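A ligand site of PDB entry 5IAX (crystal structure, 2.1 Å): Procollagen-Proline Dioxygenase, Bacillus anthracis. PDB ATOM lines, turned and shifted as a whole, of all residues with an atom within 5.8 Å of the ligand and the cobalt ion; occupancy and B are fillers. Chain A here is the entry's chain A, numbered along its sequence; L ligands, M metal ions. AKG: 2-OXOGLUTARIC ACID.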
ATOM      1  N   HIS A 115      -4.946   0.872  -9.832  1.00  0.00           N
ATOM      2  CA  HIS A 115      -3.765   0.019  -9.773  1.00  0.00           C
ATOM      3  C   HIS A 115      -2.854   0.529  -8.658  1.00  0.00           C
ATOM      4  O   HIS A 115      -2.429   1.699  -8.679  1.00  0.00           O
ATOM      5  CB  HIS A 115      -3.041  -0.003 -11.127  1.00  0.00           C
ATOM      6  CG  HIS A 115      -1.851  -0.906 -11.168  1.00  0.00           C
ATOM      7  ND1 HIS A 115      -0.567  -0.458 -10.902  1.00  0.00           N
ATOM      8  CD2 HIS A 115      -1.734  -2.242 -11.399  1.00  0.00           C
ATOM      9  CE1 HIS A 115       0.278  -1.469 -10.983  1.00  0.00           C
ATOM     10  NE2 HIS A 115      -0.406  -2.569 -11.282  1.00  0.00           N
ATOM     11  N   LEU A 117       0.646   0.272  -6.381  1.00  0.00           N
ATOM     12  CA  LEU A 117       2.045  -0.119  -6.535  1.00  0.00           C
ATOM     13  C   LEU A 117       2.854   0.350  -5.341  1.00  0.00           C
ATOM     14  O   LEU A 117       2.706   1.490  -4.881  1.00  0.00           O
ATOM     15  CB  LEU A 117       2.654   0.467  -7.824  1.00  0.00           C
ATOM     16  CG  LEU A 117       4.120   0.175  -8.106  1.00  0.00           C
ATOM     17  CD1 LEU A 117       4.430  -1.315  -7.934  1.00  0.00           C
ATOM     18  CD2 LEU A 117       4.392   0.594  -9.535  1.00  0.00           C
ATOM     19  N   TYR A 119       6.811   0.646  -3.790  1.00  0.00           N
ATOM     20  CA  TYR A 119       8.261   0.597  -3.972  1.00  0.00           C
ATOM     21  C   TYR A 119       8.915   0.513  -2.605  1.00  0.00           C
ATOM     22  O   TYR A 119       8.714   1.411  -1.773  1.00  0.00           O
ATOM     23  CB  TYR A 119       8.815   1.835  -4.676  1.00  0.00           C
ATOM     24  CG  TYR A 119       8.197   2.193  -5.993  1.00  0.00           C
ATOM     25  CD1 TYR A 119       6.995   2.897  -6.052  1.00  0.00           C
ATOM     26  CD2 TYR A 119       8.839   1.895  -7.173  1.00  0.00           C
ATOM     27  CE1 TYR A 119       6.431   3.249  -7.274  1.00  0.00           C
ATOM     28  CE2 TYR A 119       8.296   2.226  -8.397  1.00  0.00           C
ATOM     29  CZ  TYR A 119       7.107   2.926  -8.438  1.00  0.00           C
ATOM     30  OH  TYR A 119       6.599   3.254  -9.666  1.00  0.00           O
ATOM     31  N   TYR A 125      10.833   2.655 -11.184  1.00  0.00           N
ATOM     32  CA  TYR A 125      10.105   2.334 -12.406  1.00  0.00           C
ATOM     33  C   TYR A 125      10.846   3.003 -13.553  1.00  0.00           C
ATOM     34  O   TYR A 125      10.796   4.228 -13.712  1.00  0.00           O
ATOM     35  CB  TYR A 125       8.650   2.814 -12.273  1.00  0.00           C
ATOM     36  CG  TYR A 125       7.629   2.224 -13.237  1.00  0.00           C
ATOM     37  CD1 TYR A 125       8.017   1.573 -14.416  1.00  0.00           C
ATOM     38  CD2 TYR A 125       6.262   2.360 -12.994  1.00  0.00           C
ATOM     39  CE1 TYR A 125       7.069   1.042 -15.327  1.00  0.00           C
ATOM     40  CE2 TYR A 125       5.310   1.838 -13.895  1.00  0.00           C
ATOM     41  CZ  TYR A 125       5.720   1.182 -15.052  1.00  0.00           C
ATOM     42  OH  TYR A 125       4.778   0.686 -15.923  1.00  0.00           O
ATOM     43  N   HIS A 128       9.310   5.024 -19.252  1.00  0.00           N
ATOM     44  CA  HIS A 128       8.479   4.240 -20.155  1.00  0.00           C
ATOM     45  C   HIS A 128       7.403   5.159 -20.674  1.00  0.00           C
ATOM     46  O   HIS A 128       7.246   6.288 -20.197  1.00  0.00           O
ATOM     47  CB  HIS A 128       7.848   3.047 -19.442  1.00  0.00           C
ATOM     48  CG  HIS A 128       7.039   3.450 -18.261  1.00  0.00           C
ATOM     49  ND1 HIS A 128       7.592   3.652 -17.015  1.00  0.00           N
ATOM     50  CD2 HIS A 128       5.726   3.790 -18.156  1.00  0.00           C
ATOM     51  CE1 HIS A 128       6.647   4.077 -16.184  1.00  0.00           C
ATOM     52  NE2 HIS A 128       5.515   4.149 -16.852  1.00  0.00           N
ATOM     53  N   TYR A 129       6.677   4.658 -21.659  1.00  0.00           N
ATOM     54  CA  TYR A 129       5.448   5.296 -22.086  1.00  0.00           C
ATOM     55  C   TYR A 129       4.288   4.533 -21.478  1.00  0.00           C
ATOM     56  O   TYR A 129       4.342   3.304 -21.373  1.00  0.00           O
ATOM     57  CB  TYR A 129       5.336   5.312 -23.607  1.00  0.00           C
ATOM     58  CG  TYR A 129       6.444   6.091 -24.309  1.00  0.00           C
ATOM     59  CD1 TYR A 129       6.511   7.480 -24.228  1.00  0.00           C
ATOM     60  CD2 TYR A 129       7.409   5.422 -25.069  1.00  0.00           C
ATOM     61  CE1 TYR A 129       7.533   8.197 -24.865  1.00  0.00           C
ATOM     62  CE2 TYR A 129       8.439   6.129 -25.704  1.00  0.00           C
ATOM     63  CZ  TYR A 129       8.483   7.517 -25.600  1.00  0.00           C
ATOM     64  OH  TYR A 129       9.477   8.216 -26.231  1.00  0.00           O
ATOM     65  N   ASP A 130       3.225   5.251 -21.069  1.00  0.00           N
ATOM     66  CA  ASP A 130       2.068   4.521 -20.570  1.00  0.00           C
ATOM     67  C   ASP A 130       1.203   3.968 -21.698  1.00  0.00           C
ATOM     68  O   ASP A 130       0.530   2.960 -21.500  1.00  0.00           O
ATOM     69  CB  ASP A 130       1.209   5.383 -19.651  1.00  0.00           C
ATOM     70  CG  ASP A 130       1.773   5.466 -18.261  1.00  0.00           C
ATOM     71  OD1 ASP A 130       2.772   4.756 -18.003  1.00  0.00           O
ATOM     72  OD2 ASP A 130       1.236   6.253 -17.442  1.00  0.00           O
ATOM     73  N   THR A 146      -3.278   9.516 -17.841  1.00  0.00           N
ATOM     74  CA  THR A 146      -2.824   8.813 -16.657  1.00  0.00           C
ATOM     75  C   THR A 146      -3.028   9.732 -15.476  1.00  0.00           C
ATOM     76  O   THR A 146      -2.850  10.944 -15.598  1.00  0.00           O
ATOM     77  CB  THR A 146      -1.311   8.446 -16.762  1.00  0.00           C
ATOM     78  OG1 THR A 146      -1.057   7.588 -17.890  1.00  0.00           O
ATOM     79  CG2 THR A 146      -0.832   7.764 -15.508  1.00  0.00           C
ATOM     80  N   VAL A 148      -1.440   9.620 -11.534  1.00  0.00           N
ATOM     81  CA  VAL A 148      -0.640   8.975 -10.483  1.00  0.00           C
ATOM     82  C   VAL A 148      -0.911   9.681  -9.161  1.00  0.00           C
ATOM     83  O   VAL A 148      -0.562  10.854  -8.984  1.00  0.00           O
ATOM     84  CB  VAL A 148       0.872   9.009 -10.807  1.00  0.00           C
ATOM     85  CG1 VAL A 148       1.664   8.482  -9.639  1.00  0.00           C
ATOM     86  CG2 VAL A 148       1.174   8.243 -12.073  1.00  0.00           C
ATOM     87  N   TYR A 150      -0.327   9.866  -5.049  1.00  0.00           N
ATOM     88  CA  TYR A 150       0.675   9.532  -4.040  1.00  0.00           C
ATOM     89  C   TYR A 150      -0.048   9.178  -2.748  1.00  0.00           C
ATOM     90  O   TYR A 150      -0.697  10.029  -2.139  1.00  0.00           O
ATOM     91  CB  TYR A 150       1.629  10.692  -3.834  1.00  0.00           C
ATOM     92  CG  TYR A 150       2.338  11.083  -5.086  1.00  0.00           C
ATOM     93  CD1 TYR A 150       3.226  10.203  -5.709  1.00  0.00           C
ATOM     94  CD2 TYR A 150       2.138  12.329  -5.659  1.00  0.00           C
ATOM     95  CE1 TYR A 150       3.878  10.559  -6.880  1.00  0.00           C
ATOM     96  CE2 TYR A 150       2.792  12.705  -6.828  1.00  0.00           C
ATOM     97  CZ  TYR A 150       3.679  11.812  -7.430  1.00  0.00           C
ATOM     98  OH  TYR A 150       4.315  12.188  -8.585  1.00  0.00           O
ATOM     99  N   GLY A 158      11.952   8.734  -5.162  1.00  0.00           N
ATOM    100  CA  GLY A 158      10.600   8.390  -5.579  1.00  0.00           C
ATOM    101  C   GLY A 158       9.866   9.411  -6.432  1.00  0.00           C
ATOM    102  O   GLY A 158       8.646   9.307  -6.572  1.00  0.00           O
ATOM    103  N   GLU A 159      10.571  10.364  -7.047  1.00  0.00           N
ATOM    104  CA  GLU A 159       9.877  11.375  -7.847  1.00  0.00           C
ATOM    105  C   GLU A 159       9.409  10.791  -9.168  1.00  0.00           C
ATOM    106  O   GLU A 159      10.030   9.877  -9.740  1.00  0.00           O
ATOM    107  CB  GLU A 159      10.753  12.613  -8.092  1.00  0.00           C
ATOM    108  CG  GLU A 159      12.166  12.379  -8.476  1.00  0.00           C
ATOM    109  CD  GLU A 159      13.056  12.220  -7.241  1.00  0.00           C
ATOM    110  OE1 GLU A 159      13.169  11.119  -6.724  1.00  0.00           O
ATOM    111  OE2 GLU A 159      13.601  13.217  -6.740  1.00  0.00           O
ATOM    112  N   THR A 160       8.281  11.293  -9.632  1.00  0.00           N
ATOM    113  CA  THR A 160       7.824  10.995 -10.982  1.00  0.00           C
ATOM    114  C   THR A 160       8.566  11.950 -11.893  1.00  0.00           C
ATOM    115  O   THR A 160       8.430  13.167 -11.748  1.00  0.00           O
ATOM    116  CB  THR A 160       6.311  11.199 -11.125  1.00  0.00           C
ATOM    117  OG1 THR A 160       5.617  10.490 -10.104  1.00  0.00           O
ATOM    118  CG2 THR A 160       5.841  10.743 -12.495  1.00  0.00           C
ATOM    119  N   PHE A 161       9.410  11.440 -12.793  1.00  0.00           N
ATOM    120  CA  PHE A 161      10.243  12.313 -13.595  1.00  0.00           C
ATOM    121  C   PHE A 161       9.967  12.084 -15.062  1.00  0.00           C
ATOM    122  O   PHE A 161       9.699  10.956 -15.498  1.00  0.00           O
ATOM    123  CB  PHE A 161      11.751  12.113 -13.308  1.00  0.00           C
ATOM    124  CG  PHE A 161      12.239  10.744 -13.700  1.00  0.00           C
ATOM    125  CD1 PHE A 161      12.039   9.663 -12.870  1.00  0.00           C
ATOM    126  CD2 PHE A 161      12.849  10.544 -14.923  1.00  0.00           C
ATOM    127  CE1 PHE A 161      12.463   8.396 -13.219  1.00  0.00           C
ATOM    128  CE2 PHE A 161      13.280   9.249 -15.294  1.00  0.00           C
ATOM    129  CZ  PHE A 161      13.077   8.184 -14.430  1.00  0.00           C
ATOM    130  N   PHE A 179      -1.359  13.562 -16.585  1.00  0.00           N
ATOM    131  CA  PHE A 179      -0.703  13.799 -17.864  1.00  0.00           C
ATOM    132  C   PHE A 179      -1.470  13.074 -18.967  1.00  0.00           C
ATOM    133  O   PHE A 179      -2.111  12.067 -18.718  1.00  0.00           O
ATOM    134  CB  PHE A 179       0.809  13.520 -17.851  1.00  0.00           C
ATOM    135  CG  PHE A 179       1.183  12.103 -17.494  1.00  0.00           C
ATOM    136  CD1 PHE A 179       1.245  11.702 -16.185  1.00  0.00           C
ATOM    137  CD2 PHE A 179       1.518  11.201 -18.482  1.00  0.00           C
ATOM    138  CE1 PHE A 179       1.617  10.419 -15.853  1.00  0.00           C
ATOM    139  CE2 PHE A 179       1.885   9.911 -18.165  1.00  0.00           C
ATOM    140  CZ  PHE A 179       1.934   9.520 -16.850  1.00  0.00           C
ATOM    141  N   HIS A 194       8.225   8.912 -18.979  1.00  0.00           N
ATOM    142  CA  HIS A 194       8.313   9.191 -17.549  1.00  0.00           C
ATOM    143  C   HIS A 194       8.681   7.928 -16.778  1.00  0.00           C
ATOM    144  O   HIS A 194       8.503   6.807 -17.258  1.00  0.00           O
ATOM    145  CB  HIS A 194       6.996   9.670 -16.996  1.00  0.00           C
ATOM    146  CG  HIS A 194       5.911   8.654 -17.123  1.00  0.00           C
ATOM    147  ND1 HIS A 194       5.236   8.446 -18.308  1.00  0.00           N
ATOM    148  CD2 HIS A 194       5.419   7.744 -16.249  1.00  0.00           C
ATOM    149  CE1 HIS A 194       4.339   7.491 -18.142  1.00  0.00           C
ATOM    150  NE2 HIS A 194       4.438   7.043 -16.897  1.00  0.00           N
ATOM    151  N   GLY A 195       9.063   8.133 -15.529  1.00  0.00           N
ATOM    152  CA  GLY A 195       9.354   7.025 -14.651  1.00  0.00           C
ATOM    153  C   GLY A 195       9.271   7.416 -13.188  1.00  0.00           C
ATOM    154  O   GLY A 195       9.076   8.582 -12.829  1.00  0.00           O
ATOM    155  N   GLY A 196       9.427   6.405 -12.349  1.00  0.00           N
ATOM    156  CA  GLY A 196       9.455   6.569 -10.925  1.00  0.00           C
ATOM    157  C   GLY A 196      10.870   6.377 -10.471  1.00  0.00           C
ATOM    158  O   GLY A 196      11.439   5.290 -10.654  1.00  0.00           O
ATOM    159  N   ALA A 197      11.474   7.445  -9.934  1.00  0.00           N
ATOM    160  CA  ALA A 197      12.871   7.423  -9.532  1.00  0.00           C
ATOM    161  C   ALA A 197      13.080   6.515  -8.320  1.00  0.00           C
ATOM    162  O   ALA A 197      12.169   6.334  -7.506  1.00  0.00           O
ATOM    163  CB  ALA A 197      13.357   8.839  -9.199  1.00  0.00           C
ATOM    164  N   LYS A 204       7.387   3.859  -1.022  1.00  0.00           N
ATOM    165  CA  LYS A 204       6.469   4.665  -1.817  1.00  0.00           C
ATOM    166  C   LYS A 204       5.269   3.821  -2.205  1.00  0.00           C
ATOM    167  O   LYS A 204       5.422   2.743  -2.770  1.00  0.00           O
ATOM    168  CB  LYS A 204       7.168   5.199  -3.075  1.00  0.00           C
ATOM    169  CG  LYS A 204       6.256   5.910  -4.088  1.00  0.00           C
ATOM    170  CD  LYS A 204       7.117   6.573  -5.185  1.00  0.00           C
ATOM    171  CE  LYS A 204       6.339   6.789  -6.470  1.00  0.00           C
ATOM    172  NZ  LYS A 204       7.194   7.263  -7.584  1.00  0.00           N
ATOM    173  N   ILE A 206       1.624   4.185  -4.436  1.00  0.00           N
ATOM    174  CA  ILE A 206       0.857   4.959  -5.404  1.00  0.00           C
ATOM    175  C   ILE A 206      -0.356   4.185  -5.860  1.00  0.00           C
ATOM    176  O   ILE A 206      -0.402   2.942  -5.830  1.00  0.00           O
ATOM    177  CB  ILE A 206       1.674   5.363  -6.666  1.00  0.00           C
ATOM    178  CG1 ILE A 206       2.247   4.137  -7.387  1.00  0.00           C
ATOM    179  CG2 ILE A 206       2.760   6.444  -6.320  1.00  0.00           C
ATOM    180  CD1 ILE A 206       2.865   4.463  -8.792  1.00  0.00           C
ATOM    181  N   THR A 208      -2.503   4.273  -9.550  1.00  0.00           N
ATOM    182  CA  THR A 208      -2.536   4.798 -10.903  1.00  0.00           C
ATOM    183  C   THR A 208      -3.881   4.481 -11.551  1.00  0.00           C
ATOM    184  O   THR A 208      -4.396   3.371 -11.448  1.00  0.00           O
ATOM    185  CB  THR A 208      -1.387   4.244 -11.728  1.00  0.00           C
ATOM    186  OG1 THR A 208      -0.170   4.484 -11.028  1.00  0.00           O
ATOM    187  CG2 THR A 208      -1.299   4.940 -13.073  1.00  0.00           C
ATOM    188  N   TRP A 210      -5.099   4.410 -15.316  1.00  0.00           N
ATOM    189  CA  TRP A 210      -4.854   4.557 -16.745  1.00  0.00           C
ATOM    190  C   TRP A 210      -6.204   4.602 -17.459  1.00  0.00           C
ATOM    191  O   TRP A 210      -7.077   3.775 -17.192  1.00  0.00           O
ATOM    192  CB  TRP A 210      -3.993   3.407 -17.279  1.00  0.00           C
ATOM    193  CG  TRP A 210      -2.604   3.350 -16.670  1.00  0.00           C
ATOM    194  CD1 TRP A 210      -1.604   4.238 -16.856  1.00  0.00           C
ATOM    195  CD2 TRP A 210      -2.082   2.316 -15.802  1.00  0.00           C
ATOM    196  NE1 TRP A 210      -0.490   3.841 -16.155  1.00  0.00           N
ATOM    197  CE2 TRP A 210      -0.751   2.674 -15.497  1.00  0.00           C
ATOM    198  CE3 TRP A 210      -2.600   1.124 -15.268  1.00  0.00           C
ATOM    199  CZ2 TRP A 210       0.079   1.889 -14.655  1.00  0.00           C
ATOM    200  CZ3 TRP A 210      -1.784   0.333 -14.445  1.00  0.00           C
ATOM    201  CH2 TRP A 210      -0.460   0.722 -14.140  1.00  0.00           C
HETATM  202  C1  AKG L   1       2.663   4.692 -13.860  1.00  0.00           C
HETATM  203  O1  AKG L   1       2.319   4.619 -15.057  1.00  0.00           O
HETATM  204  O2  AKG L   1       1.967   4.228 -12.946  1.00  0.00           O
HETATM  205  C2  AKG L   1       3.936   5.380 -13.481  1.00  0.00           C
HETATM  206  O5  AKG L   1       4.656   5.702 -14.326  1.00  0.00           O
HETATM  207  C3  AKG L   1       4.226   5.615 -11.996  1.00  0.00           C
HETATM  208  C4  AKG L   1       5.342   6.623 -11.819  1.00  0.00           C
HETATM  209  C5  AKG L   1       5.754   6.760 -10.358  1.00  0.00           C
HETATM  210  O3  AKG L   1       5.956   7.899  -9.876  1.00  0.00           O
HETATM  211  O4  AKG L   1       5.879   5.753  -9.613  1.00  0.00           O
HETATM  212 CO    CO M   1       3.777   5.229 -16.211  1.00  0.00          CO
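The side-chain hydroxyl of Tyr 119 is in hydrogen-bond range of an oxygen (O4) of the ligand (2.6 Å). The side-chain hydroxyl (OG1) of Thr 160 sits at hydrogen-bond distance from an oxygen (O3) of the ligand (2.6 Å). The side-chain amino group (NZ) of Lys 204 is in salt-bridge range of an oxygen (O3) of the ligand (2.7 Å). The side-chain hydroxyl of Thr 208 lies within hydrogen-bond range of an oxygen (O2) of the ligand (2.9 Å). NE1 of Trp 210 lies close to O1 of the ligand, 3.1 Å away.
The side-chain carboxylate (OD2) of Asp 130 sits at hydrogen-bond distance from the indole nitrogen (NE1) of Trp 210. OD2 of Asp 130 is in hydrogen-bond range of OG1 of Thr 146, at 2.7 Å. The backbone carbonyl oxygen (O) of Lys 204 lies within hydrogen-bond range of the backbone NH (N) of Tyr 119 (2.7 Å). The side-chain hydroxyl (OG1) of Thr 160 sits at hydrogen-bond distance from the side-chain hydroxyl (OH) of Tyr 150, at 2.6 Å. The side-chain amino group (NZ) of Lys 204 is in hydrogen-bond range of the backbone carbonyl oxygen (O) of Gly 158. The backbone NH (N) of Thr 208 lies within hydrogen-bond range of the backbone carbonyl oxygen (O) of His 115 (2.7 Å). O of Ile 206 lies within hydrogen-bond range of N of Leu 117 (2.9 Å). O of Gly 196 lies within hydrogen-bond range of N of Tyr 125 (2.8 Å).
Residues that only touch the ligand: Tyr 125, Gly 196 and Ile 206. Hydrophobic or aromatic side chains within 4 Å of the ligand: Tyr 119, Tyr 125, His 128, His 194, Ile 206 and Trp 210. 11 residues have an atom within 4 Å of the ligand: Tyr 119, Tyr 125, His 128, Asp 130, Thr 160, His 194, Gly 196, Lys 204, Ile 206, Thr 208 and Trp 210.
Within 4 Å of the cobalt ion: His 128, Asp 130 and His 194. Along chain A the residues within 4 Å of the cobalt ion span positions 128 to 194. The nearest printed residue that does not touch the cobalt ion is Tyr 125 (4.4 Å).
The cobalt ion is bound by O1 of the ligand. The cobalt ion is bound by a ring nitrogen (NE2) of His 194 (2.0 Å). The cobalt ion is bound by the side-chain carboxylate (OD1) of Asp 130, 2.1 Å away. An oxygen (O5) of the ligand is bound to the cobalt ion (2.1 Å). The cobalt ion is bound by a ring nitrogen (NE2) of His 128 (2.1 Å). The cobalt ion has five donor atoms within binding distance.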
